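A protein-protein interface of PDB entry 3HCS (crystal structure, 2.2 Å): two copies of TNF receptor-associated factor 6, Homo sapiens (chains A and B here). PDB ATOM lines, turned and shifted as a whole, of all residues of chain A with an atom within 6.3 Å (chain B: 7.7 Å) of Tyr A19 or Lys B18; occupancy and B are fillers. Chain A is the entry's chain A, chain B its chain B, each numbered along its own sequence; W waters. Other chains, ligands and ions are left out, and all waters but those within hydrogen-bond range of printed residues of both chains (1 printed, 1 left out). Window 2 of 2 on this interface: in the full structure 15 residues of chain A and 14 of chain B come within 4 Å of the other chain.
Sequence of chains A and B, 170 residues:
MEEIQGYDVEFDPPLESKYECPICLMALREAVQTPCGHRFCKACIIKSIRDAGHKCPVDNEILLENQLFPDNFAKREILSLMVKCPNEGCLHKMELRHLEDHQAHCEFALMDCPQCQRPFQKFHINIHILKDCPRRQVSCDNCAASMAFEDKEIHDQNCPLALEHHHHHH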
ATOM      1  N   LEU A  15      27.173  -2.096  13.063  1.00  0.00           N
ATOM      2  CA  LEU A  15      26.043  -2.882  13.529  1.00  0.00           C
ATOM      3  C   LEU A  15      25.192  -3.348  12.357  1.00  0.00           C
ATOM      4  O   LEU A  15      24.923  -2.583  11.433  1.00  0.00           O
ATOM      5  CB  LEU A  15      25.179  -2.053  14.479  1.00  0.00           C
ATOM      6  CG  LEU A  15      24.031  -2.790  15.175  1.00  0.00           C
ATOM      7  CD1 LEU A  15      24.584  -3.882  16.073  1.00  0.00           C
ATOM      8  CD2 LEU A  15      23.226  -1.808  15.995  1.00  0.00           C
ATOM      9  N   GLU A  16      24.780  -4.609  12.396  1.00  0.00           N
ATOM     10  CA  GLU A  16      23.942  -5.175  11.348  1.00  0.00           C
ATOM     11  C   GLU A  16      22.494  -4.751  11.613  1.00  0.00           C
ATOM     12  O   GLU A  16      22.077  -4.604  12.762  1.00  0.00           O
ATOM     13  CB  GLU A  16      24.051  -6.701  11.356  1.00  0.00           C
ATOM     14  CG  GLU A  16      25.483  -7.217  11.271  1.00  0.00           C
ATOM     15  CD  GLU A  16      25.607  -8.674  11.697  1.00  0.00           C
ATOM     16  OE1 GLU A  16      25.093  -9.554  10.972  1.00  0.00           O
ATOM     17  OE2 GLU A  16      26.214  -8.935  12.764  1.00  0.00           O
ATOM     18  N   SER A  17      21.735  -4.546  10.544  1.00  0.00           N
ATOM     19  CA  SER A  17      20.343  -4.126  10.662  1.00  0.00           C
ATOM     20  C   SER A  17      19.476  -5.056  11.511  1.00  0.00           C
ATOM     21  O   SER A  17      18.536  -4.604  12.153  1.00  0.00           O
ATOM     22  CB  SER A  17      19.725  -3.982   9.267  1.00  0.00           C
ATOM     23  OG  SER A  17      19.788  -5.204   8.554  1.00  0.00           O
ATOM     24  N   LYS A  18      19.786  -6.349  11.511  1.00  0.00           N
ATOM     25  CA  LYS A  18      19.012  -7.318  12.286  1.00  0.00           C
ATOM     26  C   LYS A  18      19.060  -7.084  13.798  1.00  0.00           C
ATOM     27  O   LYS A  18      18.250  -7.641  14.544  1.00  0.00           O
ATOM     28  CB  LYS A  18      19.487  -8.741  11.975  1.00  0.00           C
ATOM     29  CG  LYS A  18      20.976  -8.967  12.202  1.00  0.00           C
ATOM     30  CD  LYS A  18      21.343 -10.439  12.051  1.00  0.00           C
ATOM     31  CE  LYS A  18      20.671 -11.288  13.122  1.00  0.00           C
ATOM     32  NZ  LYS A  18      21.020 -12.730  12.987  1.00  0.00           N
ATOM     33  N   TYR A  19      20.006  -6.267  14.247  1.00  0.00           N
ATOM     34  CA  TYR A  19      20.152  -5.978  15.664  1.00  0.00           C
ATOM     35  C   TYR A  19      19.690  -4.568  16.003  1.00  0.00           C
ATOM     36  O   TYR A  19      19.798  -4.118  17.146  1.00  0.00           O
ATOM     37  CB  TYR A  19      21.606  -6.171  16.082  1.00  0.00           C
ATOM     38  CG  TYR A  19      22.090  -7.585  15.879  1.00  0.00           C
ATOM     39  CD1 TYR A  19      21.391  -8.662  16.419  1.00  0.00           C
ATOM     40  CD2 TYR A  19      23.240  -7.850  15.139  1.00  0.00           C
ATOM     41  CE1 TYR A  19      21.825  -9.971  16.226  1.00  0.00           C
ATOM     42  CE2 TYR A  19      23.684  -9.153  14.941  1.00  0.00           C
ATOM     43  CZ  TYR A  19      22.974 -10.208  15.486  1.00  0.00           C
ATOM     44  OH  TYR A  19      23.417 -11.496  15.300  1.00  0.00           O
ATOM     45  N   GLU A  20      19.167  -3.873  15.002  1.00  0.00           N
ATOM     46  CA  GLU A  20      18.674  -2.516  15.194  1.00  0.00           C
ATOM     47  C   GLU A  20      17.198  -2.506  15.574  1.00  0.00           C
ATOM     48  O   GLU A  20      16.407  -3.306  15.076  1.00  0.00           O
ATOM     49  CB  GLU A  20      18.847  -1.688  13.920  1.00  0.00           C
ATOM     50  CG  GLU A  20      20.255  -1.206  13.667  1.00  0.00           C
ATOM     51  CD  GLU A  20      20.383  -0.458  12.350  1.00  0.00           C
ATOM     52  OE1 GLU A  20      19.650   0.541  12.153  1.00  0.00           O
ATOM     53  OE2 GLU A  20      21.218  -0.874  11.514  1.00  0.00           O
ATOM     54  N   CYS A  21      16.832  -1.600  16.469  1.00  0.00           N
ATOM     55  CA  CYS A  21      15.451  -1.474  16.883  1.00  0.00           C
ATOM     56  C   CYS A  21      14.701  -0.632  15.853  1.00  0.00           C
ATOM     57  O   CYS A  21      15.097   0.493  15.550  1.00  0.00           O
ATOM     58  CB  CYS A  21      15.363  -0.797  18.238  1.00  0.00           C
ATOM     59  SG  CYS A  21      13.672  -0.491  18.705  1.00  0.00           S
ATOM     60  N   MET A  26      18.565   2.053  16.879  1.00  0.00           N
ATOM     61  CA  MET A  26      19.876   1.787  17.463  1.00  0.00           C
ATOM     62  C   MET A  26      19.908   0.339  17.956  1.00  0.00           C
ATOM     63  O   MET A  26      18.886  -0.346  17.935  1.00  0.00           O
ATOM     64  CB  MET A  26      20.146   2.753  18.610  1.00  0.00           C
ATOM     65  CG  MET A  26      20.137   4.203  18.170  1.00  0.00           C
ATOM     66  SD  MET A  26      20.689   5.310  19.467  1.00  0.00           S
ATOM     67  CE  MET A  26      19.194   5.421  20.498  1.00  0.00           C
ATOM     68  N   ALA A  27      21.076  -0.132  18.385  1.00  0.00           N
ATOM     69  CA  ALA A  27      21.205  -1.498  18.874  1.00  0.00           C
ATOM     70  C   ALA A  27      20.190  -1.767  19.983  1.00  0.00           C
ATOM     71  O   ALA A  27      20.051  -0.979  20.918  1.00  0.00           O
ATOM     72  CB  ALA A  27      22.617  -1.742  19.389  1.00  0.00           C
ATOM     73  N   LEU A  28      19.482  -2.885  19.864  1.00  0.00           N
ATOM     74  CA  LEU A  28      18.472  -3.281  20.839  1.00  0.00           C
ATOM     75  C   LEU A  28      18.991  -3.314  22.280  1.00  0.00           C
ATOM     76  O   LEU A  28      20.017  -3.928  22.568  1.00  0.00           O
ATOM     77  CB  LEU A  28      17.925  -4.664  20.481  1.00  0.00           C
ATOM     78  CG  LEU A  28      17.332  -4.819  19.078  1.00  0.00           C
ATOM     79  CD1 LEU A  28      17.298  -6.291  18.710  1.00  0.00           C
ATOM     80  CD2 LEU A  28      15.947  -4.200  19.033  1.00  0.00           C
ATOM     81  N   ARG A  39      11.802  -7.693  16.658  1.00  0.00           N
ATOM     82  CA  ARG A  39      12.566  -7.320  17.841  1.00  0.00           C
ATOM     83  C   ARG A  39      12.551  -5.830  18.119  1.00  0.00           C
ATOM     84  O   ARG A  39      12.596  -5.021  17.199  1.00  0.00           O
ATOM     85  CB  ARG A  39      14.012  -7.761  17.681  1.00  0.00           C
ATOM     86  CG  ARG A  39      14.209  -9.240  17.503  1.00  0.00           C
ATOM     87  CD  ARG A  39      15.571  -9.430  16.895  1.00  0.00           C
ATOM     88  NE  ARG A  39      16.148 -10.731  17.168  1.00  0.00           N
ATOM     89  CZ  ARG A  39      17.354 -11.087  16.750  1.00  0.00           C
ATOM     90  NH1 ARG A  39      18.081 -10.229  16.046  1.00  0.00           N
ATOM     91  NH2 ARG A  39      17.834 -12.289  17.041  1.00  0.00           N
ATOM     92  N   PHE A  73      18.648 -14.357  23.396  1.00  0.00           N
ATOM     93  CA  PHE A  73      19.631 -14.790  22.423  1.00  0.00           C
ATOM     94  C   PHE A  73      20.195 -13.521  21.773  1.00  0.00           C
ATOM     95  O   PHE A  73      21.409 -13.365  21.656  1.00  0.00           O
ATOM     96  CB  PHE A  73      19.013 -15.688  21.350  1.00  0.00           C
ATOM     97  CG  PHE A  73      20.017 -16.196  20.349  1.00  0.00           C
ATOM     98  CD1 PHE A  73      20.715 -17.374  20.584  1.00  0.00           C
ATOM     99  CD2 PHE A  73      20.306 -15.461  19.202  1.00  0.00           C
ATOM    100  CE1 PHE A  73      21.696 -17.817  19.689  1.00  0.00           C
ATOM    101  CE2 PHE A  73      21.281 -15.890  18.301  1.00  0.00           C
ATOM    102  CZ  PHE A  73      21.978 -17.069  18.545  1.00  0.00           C
ATOM    103  N   ALA A  74      19.298 -12.617  21.376  1.00  0.00           N
ATOM    104  CA  ALA A  74      19.686 -11.359  20.729  1.00  0.00           C
ATOM    105  C   ALA A  74      20.518 -10.490  21.662  1.00  0.00           C
ATOM    106  O   ALA A  74      21.506  -9.878  21.249  1.00  0.00           O
ATOM    107  CB  ALA A  74      18.438 -10.591  20.287  1.00  0.00           C
ATOM    108  N   GLU A  77      24.050 -11.695  21.922  1.00  0.00           N
ATOM    109  CA  GLU A  77      24.786 -11.365  20.703  1.00  0.00           C
ATOM    110  C   GLU A  77      25.223  -9.906  20.713  1.00  0.00           C
ATOM    111  O   GLU A  77      26.396  -9.587  20.500  1.00  0.00           O
ATOM    112  CB  GLU A  77      23.929 -11.590  19.451  1.00  0.00           C
ATOM    113  CG  GLU A  77      23.677 -13.045  19.085  1.00  0.00           C
ATOM    114  CD  GLU A  77      23.150 -13.201  17.657  1.00  0.00           C
ATOM    115  OE1 GLU A  77      22.124 -12.569  17.316  1.00  0.00           O
ATOM    116  OE2 GLU A  77      23.767 -13.958  16.874  1.00  0.00           O
ATOM    117  N   ILE A  78      24.268  -9.019  20.955  1.00  0.00           N
ATOM    118  CA  ILE A  78      24.555  -7.598  20.966  1.00  0.00           C
ATOM    119  C   ILE A  78      25.629  -7.210  21.988  1.00  0.00           C
ATOM    120  O   ILE A  78      26.513  -6.408  21.680  1.00  0.00           O
ATOM    121  CB  ILE A  78      23.263  -6.779  21.216  1.00  0.00           C
ATOM    122  CG1 ILE A  78      22.282  -7.003  20.061  1.00  0.00           C
ATOM    123  CG2 ILE A  78      23.585  -5.301  21.330  1.00  0.00           C
ATOM    124  CD1 ILE A  78      21.024  -6.151  20.115  1.00  0.00           C
ATOM    125  N   LEU A  81      29.209  -7.780  20.846  1.00  0.00           N
ATOM    126  CA  LEU A  81      29.687  -7.016  19.696  1.00  0.00           C
ATOM    127  C   LEU A  81      30.786  -6.016  20.065  1.00  0.00           C
ATOM    128  O   LEU A  81      30.681  -5.302  21.060  1.00  0.00           O
ATOM    129  CB  LEU A  81      28.525  -6.270  19.040  1.00  0.00           C
ATOM    130  CG  LEU A  81      27.462  -7.111  18.324  1.00  0.00           C
ATOM    131  CD1 LEU A  81      26.365  -6.209  17.793  1.00  0.00           C
ATOM    132  CD2 LEU A  81      28.103  -7.882  17.180  1.00  0.00           C
ATOM    133  N   LEU B  15      25.476 -21.764   6.163  1.00  0.00           N
ATOM    134  CA  LEU B  15      24.663 -21.428   7.324  1.00  0.00           C
ATOM    135  C   LEU B  15      25.523 -20.943   8.483  1.00  0.00           C
ATOM    136  O   LEU B  15      26.541 -21.550   8.806  1.00  0.00           O
ATOM    137  CB  LEU B  15      23.880 -22.658   7.776  1.00  0.00           C
ATOM    138  CG  LEU B  15      22.941 -22.478   8.973  1.00  0.00           C
ATOM    139  CD1 LEU B  15      21.642 -21.843   8.512  1.00  0.00           C
ATOM    140  CD2 LEU B  15      22.667 -23.824   9.610  1.00  0.00           C
ATOM    141  N   GLU B  16      25.111 -19.852   9.115  1.00  0.00           N
ATOM    142  CA  GLU B  16      25.851 -19.326  10.251  1.00  0.00           C
ATOM    143  C   GLU B  16      25.472 -20.131  11.500  1.00  0.00           C
ATOM    144  O   GLU B  16      24.327 -20.573  11.638  1.00  0.00           O
ATOM    145  CB  GLU B  16      25.539 -17.840  10.437  1.00  0.00           C
ATOM    146  CG  GLU B  16      25.965 -16.989   9.247  1.00  0.00           C
ATOM    147  CD  GLU B  16      25.729 -15.504   9.461  1.00  0.00           C
ATOM    148  OE1 GLU B  16      24.572 -15.109   9.706  1.00  0.00           O
ATOM    149  OE2 GLU B  16      26.703 -14.729   9.378  1.00  0.00           O
ATOM    150  N   SER B  17      26.440 -20.324  12.395  1.00  0.00           N
ATOM    151  CA  SER B  17      26.230 -21.087  13.621  1.00  0.00           C
ATOM    152  C   SER B  17      25.030 -20.615  14.444  1.00  0.00           C
ATOM    153  O   SER B  17      24.328 -21.424  15.046  1.00  0.00           O
ATOM    154  CB  SER B  17      27.498 -21.039  14.475  1.00  0.00           C
ATOM    155  OG  SER B  17      27.955 -19.706  14.598  1.00  0.00           O
ATOM    156  N   LYS B  18      24.784 -19.311  14.448  1.00  0.00           N
ATOM    157  CA  LYS B  18      23.673 -18.725  15.202  1.00  0.00           C
ATOM    158  C   LYS B  18      22.304 -19.302  14.823  1.00  0.00           C
ATOM    159  O   LYS B  18      21.342 -19.207  15.588  1.00  0.00           O
ATOM    160  CB  LYS B  18      23.624 -17.215  14.963  1.00  0.00           C
ATOM    161  CG  LYS B  18      23.103 -16.855  13.574  1.00  0.00           C
ATOM    162  CD  LYS B  18      22.883 -15.361  13.380  1.00  0.00           C
ATOM    163  CE  LYS B  18      24.191 -14.594  13.314  1.00  0.00           C
ATOM    164  NZ  LYS B  18      23.949 -13.184  12.899  1.00  0.00           N
ATOM    165  N   TYR B  19      22.213 -19.882  13.635  1.00  0.00           N
ATOM    166  CA  TYR B  19      20.948 -20.433  13.179  1.00  0.00           C
ATOM    167  C   TYR B  19      20.919 -21.945  13.205  1.00  0.00           C
ATOM    168  O   TYR B  19      19.985 -22.565  12.697  1.00  0.00           O
ATOM    169  CB  TYR B  19      20.631 -19.925  11.772  1.00  0.00           C
ATOM    170  CG  TYR B  19      20.337 -18.440  11.713  1.00  0.00           C
ATOM    171  CD1 TYR B  19      19.403 -17.858  12.578  1.00  0.00           C
ATOM    172  CD2 TYR B  19      20.982 -17.614  10.787  1.00  0.00           C
ATOM    173  CE1 TYR B  19      19.119 -16.489  12.521  1.00  0.00           C
ATOM    174  CE2 TYR B  19      20.705 -16.244  10.721  1.00  0.00           C
ATOM    175  CZ  TYR B  19      19.771 -15.689  11.590  1.00  0.00           C
ATOM    176  OH  TYR B  19      19.479 -14.345  11.511  1.00  0.00           O
ATOM    177  N   GLU B  20      21.943 -22.527  13.815  1.00  0.00           N
ATOM    178  CA  GLU B  20      22.067 -23.971  13.919  1.00  0.00           C
ATOM    179  C   GLU B  20      21.527 -24.473  15.262  1.00  0.00           C
ATOM    180  O   GLU B  20      21.757 -23.863  16.304  1.00  0.00           O
ATOM    181  CB  GLU B  20      23.540 -24.342  13.751  1.00  0.00           C
ATOM    182  CG  GLU B  20      23.824 -25.819  13.703  1.00  0.00           C
ATOM    183  CD  GLU B  20      25.290 -26.098  13.454  1.00  0.00           C
ATOM    184  OE1 GLU B  20      25.809 -25.635  12.414  1.00  0.00           O
ATOM    185  OE2 GLU B  20      25.918 -26.777  14.297  1.00  0.00           O
ATOM    186  N   CYS B  21      20.806 -25.586  15.229  1.00  0.00           N
ATOM    187  CA  CYS B  21      20.242 -26.169  16.439  1.00  0.00           C
ATOM    188  C   CYS B  21      21.325 -26.939  17.184  1.00  0.00           C
ATOM    189  O   CYS B  21      21.943 -27.837  16.629  1.00  0.00           O
ATOM    190  CB  CYS B  21      19.095 -27.114  16.076  1.00  0.00           C
ATOM    191  SG  CYS B  21      18.545 -28.181  17.427  1.00  0.00           S
ATOM    192  N   PRO B  22      21.570 -26.592  18.455  1.00  0.00           N
ATOM    193  CA  PRO B  22      22.594 -27.283  19.240  1.00  0.00           C
ATOM    194  C   PRO B  22      22.384 -28.797  19.307  1.00  0.00           C
ATOM    195  O   PRO B  22      23.339 -29.561  19.435  1.00  0.00           O
ATOM    196  CB  PRO B  22      22.474 -26.617  20.609  1.00  0.00           C
ATOM    197  CG  PRO B  22      22.083 -25.235  20.255  1.00  0.00           C
ATOM    198  CD  PRO B  22      21.016 -25.458  19.212  1.00  0.00           C
ATOM    199  N   LEU B  28      17.640 -24.429  12.275  1.00  0.00           N
ATOM    200  CA  LEU B  28      16.464 -24.492  13.136  1.00  0.00           C
ATOM    201  C   LEU B  28      15.143 -24.629  12.372  1.00  0.00           C
ATOM    202  O   LEU B  28      14.836 -23.812  11.507  1.00  0.00           O
ATOM    203  CB  LEU B  28      16.415 -23.228  14.006  1.00  0.00           C
ATOM    204  CG  LEU B  28      17.628 -23.010  14.921  1.00  0.00           C
ATOM    205  CD1 LEU B  28      17.756 -21.537  15.275  1.00  0.00           C
ATOM    206  CD2 LEU B  28      17.485 -23.875  16.168  1.00  0.00           C
ATOM    207  N   ARG B  39      18.348 -21.171  21.297  1.00  0.00           N
ATOM    208  CA  ARG B  39      17.424 -21.572  20.238  1.00  0.00           C
ATOM    209  C   ARG B  39      17.528 -23.058  19.922  1.00  0.00           C
ATOM    210  O   ARG B  39      18.610 -23.635  19.971  1.00  0.00           O
ATOM    211  CB  ARG B  39      17.727 -20.803  18.952  1.00  0.00           C
ATOM    212  CG  ARG B  39      17.548 -19.311  19.014  1.00  0.00           C
ATOM    213  CD  ARG B  39      18.185 -18.663  17.793  1.00  0.00           C
ATOM    214  NE  ARG B  39      17.790 -17.268  17.633  1.00  0.00           N
ATOM    215  CZ  ARG B  39      18.328 -16.440  16.744  1.00  0.00           C
ATOM    216  NH1 ARG B  39      19.288 -16.863  15.934  1.00  0.00           N
ATOM    217  NH2 ARG B  39      17.900 -15.191  16.657  1.00  0.00           N
ATOM    218  N   ASP B  71      10.336 -18.537  18.286  1.00  0.00           N
ATOM    219  CA  ASP B  71      11.259 -17.495  17.844  1.00  0.00           C
ATOM    220  C   ASP B  71      10.981 -17.247  16.375  1.00  0.00           C
ATOM    221  O   ASP B  71      11.740 -17.684  15.511  1.00  0.00           O
ATOM    222  CB  ASP B  71      12.721 -17.934  18.025  1.00  0.00           C
ATOM    223  CG  ASP B  71      13.714 -16.761  17.912  1.00  0.00           C
ATOM    224  OD1 ASP B  71      13.445 -15.784  17.181  1.00  0.00           O
ATOM    225  OD2 ASP B  71      14.785 -16.825  18.552  1.00  0.00           O
ATOM    226  N   PHE B  73      11.271 -14.576  14.789  1.00  0.00           N
ATOM    227  CA  PHE B  73      12.230 -13.688  14.147  1.00  0.00           C
ATOM    228  C   PHE B  73      13.271 -14.601  13.470  1.00  0.00           C
ATOM    229  O   PHE B  73      13.638 -14.404  12.302  1.00  0.00           O
ATOM    230  CB  PHE B  73      12.945 -12.793  15.161  1.00  0.00           C
ATOM    231  CG  PHE B  73      13.922 -11.832  14.526  1.00  0.00           C
ATOM    232  CD1 PHE B  73      13.502 -10.588  14.078  1.00  0.00           C
ATOM    233  CD2 PHE B  73      15.247 -12.198  14.329  1.00  0.00           C
ATOM    234  CE1 PHE B  73      14.384  -9.724  13.441  1.00  0.00           C
ATOM    235  CE2 PHE B  73      16.141 -11.344  13.692  1.00  0.00           C
ATOM    236  CZ  PHE B  73      15.707 -10.100  13.245  1.00  0.00           C
ATOM    237  N   ALA B  74      13.741 -15.601  14.219  1.00  0.00           N
ATOM    238  CA  ALA B  74      14.731 -16.551  13.708  1.00  0.00           C
ATOM    239  C   ALA B  74      14.165 -17.361  12.537  1.00  0.00           C
ATOM    240  O   ALA B  74      14.848 -17.584  11.531  1.00  0.00           O
ATOM    241  CB  ALA B  74      15.191 -17.490  14.826  1.00  0.00           C
ATOM    242  N   GLU B  77      14.109 -15.368   9.344  1.00  0.00           N
ATOM    243  CA  GLU B  77      15.463 -15.228   8.829  1.00  0.00           C
ATOM    244  C   GLU B  77      15.909 -16.502   8.120  1.00  0.00           C
ATOM    245  O   GLU B  77      16.434 -16.464   7.003  1.00  0.00           O
ATOM    246  CB  GLU B  77      16.437 -14.930   9.976  1.00  0.00           C
ATOM    247  CG  GLU B  77      16.215 -13.582  10.646  1.00  0.00           C
ATOM    248  CD  GLU B  77      16.692 -12.415   9.797  1.00  0.00           C
ATOM    249  OE1 GLU B  77      17.930 -12.275   9.635  1.00  0.00           O
ATOM    250  OE2 GLU B  77      15.839 -11.644   9.292  1.00  0.00           O
ATOM    251  N   ILE B  78      15.712 -17.631   8.783  1.00  0.00           N
ATOM    252  CA  ILE B  78      16.122 -18.900   8.215  1.00  0.00           C
ATOM    253  C   ILE B  78      15.398 -19.232   6.910  1.00  0.00           C
ATOM    254  O   ILE B  78      16.015 -19.763   5.984  1.00  0.00           O
ATOM    255  CB  ILE B  78      15.934 -20.027   9.245  1.00  0.00           C
ATOM    256  CG1 ILE B  78      16.865 -19.764  10.437  1.00  0.00           C
ATOM    257  CG2 ILE B  78      16.255 -21.377   8.628  1.00  0.00           C
ATOM    258  CD1 ILE B  78      16.710 -20.730  11.593  1.00  0.00           C
HETATM  259  O   HOH W   1      16.031 -14.292  18.265  1.00  0.00           O
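The side-chain amino group (NZ) of Lys B18 lies within salt-bridge range of the side-chain carboxylate (OE1) of Glu B16. The backbone carbonyl oxygen (O) of Lys B18 lies within hydrogen-bond range of the guanidinium group (NH1) of Arg B39, 3.1 Å away. N of Leu B28 lies within hydrogen-bond range of O of Tyr B19 (3.0 Å). The guanidinium group (NE) of Arg B39 is in salt-bridge range of the side-chain carboxylate (OD2) of Asp B71, at 3.2 Å. O of Lys A18 is in hydrogen-bond range of NH1 of Arg A39 (3.0 Å). OH of Tyr B19 sits at hydrogen-bond distance from OE1 of Glu B77 (3.2 Å).
Lys A18 touches its own counterpart, Lys B18. Lys A18 touches Phe B73, and with the chains exchanged Phe A73 touches Lys B18. Arg A39 touches its own counterpart, Arg B39. Glu A77 touches Lys B18, but with the chains exchanged Lys A18 does not touch Glu B77 (4.5 Å). 13 positions are printed for both chains. Of the 9 pairs that touch across the chains among the printed residues, 8 have their exchanged pair printed and touching as well.
Tyr A19 touches just one residue of chain B: Lys B18. Lys B18 touches four residues of chain A. Of the printed residues of chain B, Lys A18 touches Lys B18 (3.0 Å), Tyr B19 (2.7 Å) and Phe B73 (3.8 Å). Of the printed residues of chain B, Arg A39 touches Arg B39 (2.9 Å) and Phe B73 (3.2 Å). Printed residues of chain A within 4 Å of Tyr B19: Lys A18. Printed residues of chain A within 4 Å of Phe B73: Lys A18 and Arg A39. Leu A81 touches none of the printed residues of chain B. Asp B71 touches none of the printed residues of chain A. The nearest residue of chain B that does not touch Tyr A19 is Phe B73 (5.8 Å). The nearest residue of chain A that does not touch Lys B18 is Glu A16 (4.3 Å).
Water W1 lies within hydrogen-bond range of the guanidinium group (NH2) of Arg B39 (2.6 Å), the side-chain carboxylate (OD2) of Asp B71 (2.8 Å) and the guanidinium group (NH2) of Arg A39 (3.0 Å).
Printed residues of chain B that touch a printed residue of chain A: Lys B18, Tyr B19, Arg B39 and Phe B73. Hydrophobic or aromatic side chains of chain A that line the printed part of chain B: Tyr A19 and Phe A73. Among the printed residues, 9 pairs touch across the chains. Among the printed residues, no Asp or Glu carboxylate lies within 4 Å of a Lys or Arg side-chain nitrogen of the other chain.
OH of Tyr B19 lies within hydrogen-bond range of NZ of Lys A18, 2.7 Å away. NZ of Lys B18 lies close to NZ of Lys A18, at 3.0 Å. NH2 of Arg A39 lies close to NH2 of Arg B39. OH of Tyr A19 sits at hydrogen-bond distance from NZ of Lys B18 (3.0 Å).
Among the printed residues, merely in contact across the chains: Lys A18 with Phe B73 (3.8 Å), Arg A39 with Phe B73 (3.2 Å), Phe A73 with Lys B18 (3.7 Å), Phe A73 with Arg B39 (3.2 Å) and Glu A77 with Lys B18 (3.6 Å).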
